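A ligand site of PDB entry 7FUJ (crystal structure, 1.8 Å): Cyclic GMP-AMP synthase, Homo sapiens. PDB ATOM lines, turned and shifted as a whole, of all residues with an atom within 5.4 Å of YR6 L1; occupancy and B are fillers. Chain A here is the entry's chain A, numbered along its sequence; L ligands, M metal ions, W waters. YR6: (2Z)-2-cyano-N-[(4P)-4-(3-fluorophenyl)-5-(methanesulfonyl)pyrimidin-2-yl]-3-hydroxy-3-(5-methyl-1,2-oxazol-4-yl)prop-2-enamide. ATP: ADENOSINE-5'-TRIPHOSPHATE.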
ATOM      1  N   THR A  51     -24.014  29.903  18.479  1.00  0.00           N
ATOM      2  CA  THR A  51     -23.492  30.462  19.751  1.00  0.00           C
ATOM      3  C   THR A  51     -22.445  31.553  19.465  1.00  0.00           C
ATOM      4  O   THR A  51     -22.141  31.812  18.306  1.00  0.00           O
ATOM      5  CB  THR A  51     -22.893  29.348  20.622  1.00  0.00           C
ATOM      6  OG1 THR A  51     -21.795  28.725  19.931  1.00  0.00           O
ATOM      7  CG2 THR A  51     -23.915  28.315  21.015  1.00  0.00           C
ATOM      8  N   GLY A  52     -21.944  32.165  20.533  1.00  0.00           N
ATOM      9  CA  GLY A  52     -20.942  33.250  20.460  1.00  0.00           C
ATOM     10  C   GLY A  52     -21.512  34.525  19.881  1.00  0.00           C
ATOM     11  O   GLY A  52     -22.755  34.685  19.757  1.00  0.00           O
ATOM     12  N   ASP A  67     -19.422  30.937  15.540  1.00  0.00           N
ATOM     13  CA  ASP A  67     -19.271  29.817  16.489  1.00  0.00           C
ATOM     14  C   ASP A  67     -20.519  28.927  16.404  1.00  0.00           C
ATOM     15  O   ASP A  67     -21.662  29.444  16.424  1.00  0.00           O
ATOM     16  CB  ASP A  67     -18.971  30.338  17.894  1.00  0.00           C
ATOM     17  CG  ASP A  67     -17.759  31.246  17.895  1.00  0.00           C
ATOM     18  OD1 ASP A  67     -16.602  30.697  17.764  1.00  0.00           O
ATOM     19  OD2 ASP A  67     -17.951  32.488  17.973  1.00  0.00           O
ATOM     20  N   VAL A  68     -20.298  27.610  16.360  1.00  0.00           N
ATOM     21  CA  VAL A  68     -21.430  26.634  16.409  1.00  0.00           C
ATOM     22  C   VAL A  68     -21.020  25.425  17.254  1.00  0.00           C
ATOM     23  O   VAL A  68     -19.834  25.061  17.232  1.00  0.00           O
ATOM     24  CB  VAL A  68     -21.879  26.227  14.995  1.00  0.00           C
ATOM     25  CG1 VAL A  68     -22.369  27.435  14.228  1.00  0.00           C
ATOM     26  CG2 VAL A  68     -20.786  25.516  14.220  1.00  0.00           C
ATOM     27  N   MET A  69     -21.974  24.876  17.989  1.00  0.00           N
ATOM     28  CA  MET A  69     -21.834  23.598  18.728  1.00  0.00           C
ATOM     29  C   MET A  69     -22.541  22.507  17.926  1.00  0.00           C
ATOM     30  O   MET A  69     -23.689  22.728  17.471  1.00  0.00           O
ATOM     31  CB  MET A  69     -22.431  23.674  20.129  1.00  0.00           C
ATOM     32  CG  MET A  69     -21.929  24.857  20.921  1.00  0.00           C
ATOM     33  SD  MET A  69     -22.675  24.949  22.550  1.00  0.00           S
ATOM     34  CE  MET A  69     -21.666  23.787  23.458  1.00  0.00           C
ATOM     35  N   GLY A 144      -5.419  25.015  23.119  1.00  0.00           N
ATOM     36  CA  GLY A 144      -6.300  25.985  23.796  1.00  0.00           C
ATOM     37  C   GLY A 144      -7.792  25.731  23.548  1.00  0.00           C
ATOM     38  O   GLY A 144      -8.569  25.892  24.522  1.00  0.00           O
ATOM     39  N   SER A 145      -8.179  25.353  22.321  1.00  0.00           N
ATOM     40  CA  SER A 145      -9.597  25.303  21.847  1.00  0.00           C
ATOM     41  C   SER A 145     -10.135  23.872  21.785  1.00  0.00           C
ATOM     42  O   SER A 145      -9.499  22.971  21.271  1.00  0.00           O
ATOM     43  CB  SER A 145      -9.728  25.966  20.492  1.00  0.00           C
ATOM     44  OG  SER A 145     -11.103  26.182  20.167  1.00  0.00           O
ATOM     45  N   PRO A 146     -11.386  23.628  22.237  1.00  0.00           N
ATOM     46  CA  PRO A 146     -12.068  22.391  21.891  1.00  0.00           C
ATOM     47  C   PRO A 146     -12.513  22.391  20.413  1.00  0.00           C
ATOM     48  O   PRO A 146     -12.999  21.361  19.963  1.00  0.00           O
ATOM     49  CB  PRO A 146     -13.299  22.396  22.797  1.00  0.00           C
ATOM     50  CG  PRO A 146     -13.594  23.858  22.990  1.00  0.00           C
ATOM     51  CD  PRO A 146     -12.233  24.532  23.037  1.00  0.00           C
ATOM     52  N   ALA A 147     -12.378  23.520  19.710  1.00  0.00           N
ATOM     53  CA  ALA A 147     -13.026  23.749  18.395  1.00  0.00           C
ATOM     54  C   ALA A 147     -12.163  23.253  17.240  1.00  0.00           C
ATOM     55  O   ALA A 147     -10.939  23.406  17.298  1.00  0.00           O
ATOM     56  CB  ALA A 147     -13.327  25.228  18.224  1.00  0.00           C
ATOM     57  N   ASP A 159     -15.728  28.354  13.916  1.00  0.00           N
ATOM     58  CA  ASP A 159     -15.304  27.441  15.003  1.00  0.00           C
ATOM     59  C   ASP A 159     -16.441  26.474  15.231  1.00  0.00           C
ATOM     60  O   ASP A 159     -17.554  26.932  15.528  1.00  0.00           O
ATOM     61  CB  ASP A 159     -14.964  28.154  16.325  1.00  0.00           C
ATOM     62  CG  ASP A 159     -13.719  29.029  16.247  1.00  0.00           C
ATOM     63  OD1 ASP A 159     -12.870  28.738  15.344  1.00  0.00           O
ATOM     64  OD2 ASP A 159     -13.616  30.007  17.052  1.00  0.00           O
ATOM     65  N   ILE A 160     -16.176  25.178  15.075  1.00  0.00           N
ATOM     66  CA  ILE A 160     -17.132  24.083  15.381  1.00  0.00           C
ATOM     67  C   ILE A 160     -16.611  23.284  16.575  1.00  0.00           C
ATOM     68  O   ILE A 160     -15.526  22.662  16.460  1.00  0.00           O
ATOM     69  CB  ILE A 160     -17.339  23.192  14.153  1.00  0.00           C
ATOM     70  CG1 ILE A 160     -17.597  24.003  12.873  1.00  0.00           C
ATOM     71  CG2 ILE A 160     -18.443  22.194  14.469  1.00  0.00           C
ATOM     72  CD1 ILE A 160     -17.792  23.142  11.651  1.00  0.00           C
ATOM     73  N   THR A 161     -17.355  23.245  17.665  1.00  0.00           N
ATOM     74  CA  THR A 161     -17.000  22.378  18.817  1.00  0.00           C
ATOM     75  C   THR A 161     -18.018  21.252  18.913  1.00  0.00           C
ATOM     76  O   THR A 161     -19.235  21.511  18.926  1.00  0.00           O
ATOM     77  CB  THR A 161     -16.892  23.159  20.131  1.00  0.00           C
ATOM     78  OG1 THR A 161     -16.304  22.279  21.088  1.00  0.00           O
ATOM     79  CG2 THR A 161     -18.220  23.632  20.681  1.00  0.00           C
ATOM     80  N   VAL A 200     -17.313  20.047  26.457  1.00  0.00           N
ATOM     81  CA  VAL A 200     -16.526  20.210  25.212  1.00  0.00           C
ATOM     82  C   VAL A 200     -15.167  19.584  25.487  1.00  0.00           C
ATOM     83  O   VAL A 200     -14.724  19.521  26.642  1.00  0.00           O
ATOM     84  CB  VAL A 200     -16.456  21.688  24.767  1.00  0.00           C
ATOM     85  CG1 VAL A 200     -17.868  22.208  24.483  1.00  0.00           C
ATOM     86  CG2 VAL A 200     -15.752  22.565  25.804  1.00  0.00           C
ATOM     87  N   LYS A 202     -12.035  20.028  25.769  1.00  0.00           N
ATOM     88  CA  LYS A 202     -10.835  20.802  26.164  1.00  0.00           C
ATOM     89  C   LYS A 202     -10.300  20.113  27.408  1.00  0.00           C
ATOM     90  O   LYS A 202     -11.119  19.833  28.330  1.00  0.00           O
ATOM     91  CB  LYS A 202     -11.192  22.253  26.465  1.00  0.00           C
ATOM     92  CG  LYS A 202     -10.018  23.195  26.341  1.00  0.00           C
ATOM     93  CD  LYS A 202      -9.842  24.065  27.534  1.00  0.00           C
ATOM     94  CE  LYS A 202      -8.444  24.630  27.592  1.00  0.00           C
ATOM     95  NZ  LYS A 202      -8.508  26.105  27.576  1.00  0.00           N
ATOM     96  N   ARG A 216     -14.607  19.782  29.399  1.00  0.00           N
ATOM     97  CA  ARG A 216     -14.829  21.020  30.209  1.00  0.00           C
ATOM     98  C   ARG A 216     -16.286  21.453  30.070  1.00  0.00           C
ATOM     99  O   ARG A 216     -16.842  21.342  28.968  1.00  0.00           O
ATOM    100  CB  ARG A 216     -13.878  22.141  29.803  1.00  0.00           C
ATOM    101  CG  ARG A 216     -13.807  23.258  30.835  1.00  0.00           C
ATOM    102  CD  ARG A 216     -13.459  24.612  30.211  1.00  0.00           C
ATOM    103  NE  ARG A 216     -14.625  25.035  29.467  1.00  0.00           N
ATOM    104  CZ  ARG A 216     -14.639  25.604  28.266  1.00  0.00           C
ATOM    105  NH1 ARG A 216     -15.806  25.847  27.690  1.00  0.00           N
ATOM    106  NH2 ARG A 216     -13.535  25.903  27.617  1.00  0.00           N
ATOM    107  N   SER A 218     -19.504  23.652  29.373  1.00  0.00           N
ATOM    108  CA  SER A 218     -19.894  24.801  28.491  1.00  0.00           C
ATOM    109  C   SER A 218     -21.337  25.229  28.774  1.00  0.00           C
ATOM    110  O   SER A 218     -22.197  24.367  28.864  1.00  0.00           O
ATOM    111  CB  SER A 218     -19.743  24.501  27.034  1.00  0.00           C
ATOM    112  OG  SER A 218     -20.308  25.567  26.269  1.00  0.00           O
ATOM    113  N   SER A 220     -22.464  28.078  26.857  1.00  0.00           N
ATOM    114  CA  SER A 220     -22.620  28.990  25.693  1.00  0.00           C
ATOM    115  C   SER A 220     -24.103  29.214  25.364  1.00  0.00           C
ATOM    116  O   SER A 220     -24.450  30.321  24.976  1.00  0.00           O
ATOM    117  CB  SER A 220     -21.881  28.475  24.515  1.00  0.00           C
ATOM    118  OG  SER A 220     -20.528  28.353  24.841  1.00  0.00           O
ATOM    119  N   SER A 274      -8.519  36.914  26.310  1.00  0.00           N
ATOM    120  CA  SER A 274      -9.532  36.617  25.281  1.00  0.00           C
ATOM    121  C   SER A 274     -10.797  37.449  25.528  1.00  0.00           C
ATOM    122  O   SER A 274     -10.989  37.965  26.654  1.00  0.00           O
ATOM    123  CB  SER A 274      -9.859  35.154  25.303  1.00  0.00           C
ATOM    124  OG  SER A 274     -10.690  34.857  26.414  1.00  0.00           O
HETATM  125  C10 YR6 L   1     -10.192  28.877  24.903  1.00  0.00           C
HETATM  126  O14 YR6 L   1      -8.522  28.729  26.905  1.00  0.00           O
HETATM  127  C15 YR6 L   1     -10.667  29.244  23.612  1.00  0.00           C
HETATM  128  C16 YR6 L   1      -9.936  30.059  22.616  1.00  0.00           C
HETATM  129  C17 YR6 L   1      -8.712  29.627  22.088  1.00  0.00           C
HETATM  130  C18 YR6 L   1      -8.037  30.387  21.149  1.00  0.00           C
HETATM  131  C19 YR6 L   1      -8.584  31.565  20.662  1.00  0.00           C
HETATM  132  C20 YR6 L   1      -9.819  31.946  21.153  1.00  0.00           C
HETATM  133  C21 YR6 L   1     -10.501  31.240  22.121  1.00  0.00           C
HETATM  134  C24 YR6 L   1     -16.286  27.365  22.110  1.00  0.00           C
HETATM  135  C26 YR6 L   1     -17.528  27.284  21.393  1.00  0.00           C
HETATM  136  C27 YR6 L   1     -17.771  27.180  20.049  1.00  0.00           C
HETATM  137  N1  YR6 L   1     -18.016  25.911  24.748  1.00  0.00           N
HETATM  138  C2  YR6 L   1     -17.174  26.386  24.140  1.00  0.00           C
HETATM  139  C3  YR6 L   1     -16.100  26.967  23.418  1.00  0.00           C
HETATM  140  C4  YR6 L   1     -14.882  27.164  24.193  1.00  0.00           C
HETATM  141  O5  YR6 L   1     -14.822  26.768  25.366  1.00  0.00           O
HETATM  142  N6  YR6 L   1     -13.823  27.679  23.533  1.00  0.00           N
HETATM  143  C7  YR6 L   1     -12.580  28.020  24.008  1.00  0.00           C
HETATM  144  N8  YR6 L   1     -12.249  27.663  25.252  1.00  0.00           N
HETATM  145  C9  YR6 L   1     -11.045  28.069  25.660  1.00  0.00           C
HETATM  146  S11 YR6 L   1      -8.648  29.392  25.636  1.00  0.00           S
HETATM  147  C12 YR6 L   1      -7.357  28.851  24.599  1.00  0.00           C
HETATM  148  O13 YR6 L   1      -8.656  30.832  25.635  1.00  0.00           O
HETATM  149  F22 YR6 L   1     -10.378  33.086  20.681  1.00  0.00           F
HETATM  150  N23 YR6 L   1     -11.875  28.814  23.181  1.00  0.00           N
HETATM  151  O25 YR6 L   1     -15.319  27.937  21.426  1.00  0.00           O
HETATM  152  O28 YR6 L   1     -19.091  27.254  19.829  1.00  0.00           O
HETATM  153  N29 YR6 L   1     -19.751  27.433  21.059  1.00  0.00           N
HETATM  154  C30 YR6 L   1     -18.804  27.490  21.949  1.00  0.00           C
HETATM  155  C31 YR6 L   1     -16.922  26.983  18.861  1.00  0.00           C
HETATM  156  PG  ATP L   2     -15.647  37.029  19.540  1.00  0.00           P
HETATM  157  O1G ATP L   2     -15.591  35.799  18.659  1.00  0.00           O
HETATM  158  O2G ATP L   2     -14.328  37.375  20.186  1.00  0.00           O
HETATM  159  O3G ATP L   2     -16.359  38.193  18.927  1.00  0.00           O
HETATM  160  PB  ATP L   2     -17.155  35.132  21.177  1.00  0.00           P
HETATM  161  O1B ATP L   2     -17.983  35.142  22.411  1.00  0.00           O
HETATM  162  O2B ATP L   2     -17.787  34.626  19.893  1.00  0.00           O
HETATM  163  O3B ATP L   2     -16.614  36.592  20.812  1.00  0.00           O
HETATM  164  PA  ATP L   2     -15.114  32.990  20.936  1.00  0.00           P
HETATM  165  O1A ATP L   2     -13.681  32.992  21.339  1.00  0.00           O
HETATM  166  O2A ATP L   2     -15.486  32.858  19.479  1.00  0.00           O
HETATM  167  O3A ATP L   2     -15.768  34.377  21.404  1.00  0.00           O
HETATM  168  O5' ATP L   2     -15.874  31.921  21.806  1.00  0.00           O
HETATM  169  C5' ATP L   2     -17.186  31.419  21.412  1.00  0.00           C
HETATM  170  C4' ATP L   2     -17.951  31.066  22.654  1.00  0.00           C
HETATM  171  O4' ATP L   2     -17.299  29.957  23.317  1.00  0.00           O
HETATM  172  C3' ATP L   2     -18.040  32.148  23.734  1.00  0.00           C
HETATM  173  O3' ATP L   2     -19.074  33.112  23.592  1.00  0.00           O
HETATM  174  C2' ATP L   2     -18.268  31.299  24.999  1.00  0.00           C
HETATM  175  O2' ATP L   2     -19.602  30.921  25.165  1.00  0.00           O
HETATM  176  C1' ATP L   2     -17.384  30.085  24.728  1.00  0.00           C
HETATM  177  N9  ATP L   2     -16.047  30.222  25.302  1.00  0.00           N
HETATM  178  C8  ATP L   2     -14.910  30.805  24.757  1.00  0.00           C
HETATM  179  N7  ATP L   2     -13.893  30.815  25.581  1.00  0.00           N
HETATM  180  C5  ATP L   2     -14.364  30.169  26.729  1.00  0.00           C
HETATM  181  C6  ATP L   2     -13.742  29.833  27.952  1.00  0.00           C
HETATM  182  N6  ATP L   2     -12.470  30.112  28.251  1.00  0.00           N
HETATM  183  N1  ATP L   2     -14.490  29.178  28.859  1.00  0.00           N
HETATM  184  C2  ATP L   2     -15.762  28.890  28.558  1.00  0.00           C
HETATM  185  N3  ATP L   2     -16.457  29.177  27.456  1.00  0.00           N
HETATM  186  C4  ATP L   2     -15.677  29.806  26.567  1.00  0.00           C
HETATM  187 MG    MG M   1     -14.699  31.285  18.197  1.00  0.00          MG
HETATM  188  O   HOH W   1      -7.606  32.845  26.902  1.00  0.00           O
HETATM  189  O   HOH W   2     -12.840  32.064  18.659  1.00  0.00           O
HETATM  190  O   HOH W   3      -8.186  35.099  21.831  1.00  0.00           O
HETATM  191  O   HOH W   4     -11.550  32.121  25.307  1.00  0.00           O
HETATM  192  O   HOH W   5     -14.441  30.023  19.836  1.00  0.00           O
HETATM  193  O   HOH W   6     -12.289  35.581  20.067  1.00  0.00           O
HETATM  194  O   HOH W   7      -6.813  27.448  29.210  1.00  0.00           O
HETATM  195  O   HOH W   8     -12.133  28.697  20.218  1.00  0.00           O
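The backbone carbonyl oxygen (O) of Asp 67 is in hydrogen-bond range of the backbone NH (N) of Thr 51 (3.2 Å).
The backbone carbonyl oxygen of Val 200 is in hydrogen-bond range of the backbone NH of Arg 216 (2.8 Å).
The side-chain amino group of Lys 202 is in hydrogen-bond range of the backbone carbonyl oxygen of Gly 144 (3.1 Å).
The side-chain hydroxyl (OG) of Ser 218 is in hydrogen-bond range of the side-chain hydroxyl (OG) of Ser 220, 3.1 Å away.
The backbone carbonyl oxygen (O) of Asp 159 lies within hydrogen-bond range of the backbone NH (N) of Val 68 (2.9 Å).
The backbone carbonyl oxygen (O) of Val 68 sits at hydrogen-bond distance from the backbone NH (N) of Thr 161, 3.1 Å away.
An oxygen (O4') of ATP L2 sits close to an oxygen (O25) of YR6 L1.
Water W5 bridges an oxygen (O25) of YR6 L1 (2.8 Å) and an oxygen (O5') of ATP L2 (3.1 Å).
Water W8 bridges OG of Ser 145 (2.7 Å) and N23 of YR6 L1 (3.0 Å).
Water W7 lies within hydrogen-bond range of the side-chain amino group of Lys 202 (2.7 Å) and an oxygen (O14) of YR6 L1 (3.1 Å).
Water W4 lies within hydrogen-bond range of N7 of ATP L2, OG of Ser 274 and O13 of YR6 L1.
O of Val 68 sits close to O28 of YR6 L1.
The backbone carbonyl oxygen (O) of Gly 144 lies close to a sulfur (S11) of YR6 L1 (3.7 Å).
Merely in contact with YR6 L1: Met 69, Asp 159, Ser 220, Pro 146, Thr 161, Asp 67 and Val 200.
Of the 18 residues printed, 13 come within 4 Å of YR6 L1.
A nitrogen (N29) of YR6 L1 is in hydrogen-bond range of the side-chain hydroxyl (OG1) of Thr 51, 2.7 Å away.
An oxygen (O5) of YR6 L1 lies within hydrogen-bond range of the guanidinium group (NH1) of Arg 216 (2.7 Å).
NZ of Lys 202 sits at hydrogen-bond distance from O14 of YR6 L1 (2.7 Å).
A nitrogen (N1) of YR6 L1 sits at hydrogen-bond distance from the side-chain hydroxyl of Ser 218 (2.8 Å).
NH1 of Arg 216 sits close to N3 of ATP L2 (3.4 Å).
OG of Ser 220 sits at hydrogen-bond distance from O2' of ATP L2 (2.7 Å).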
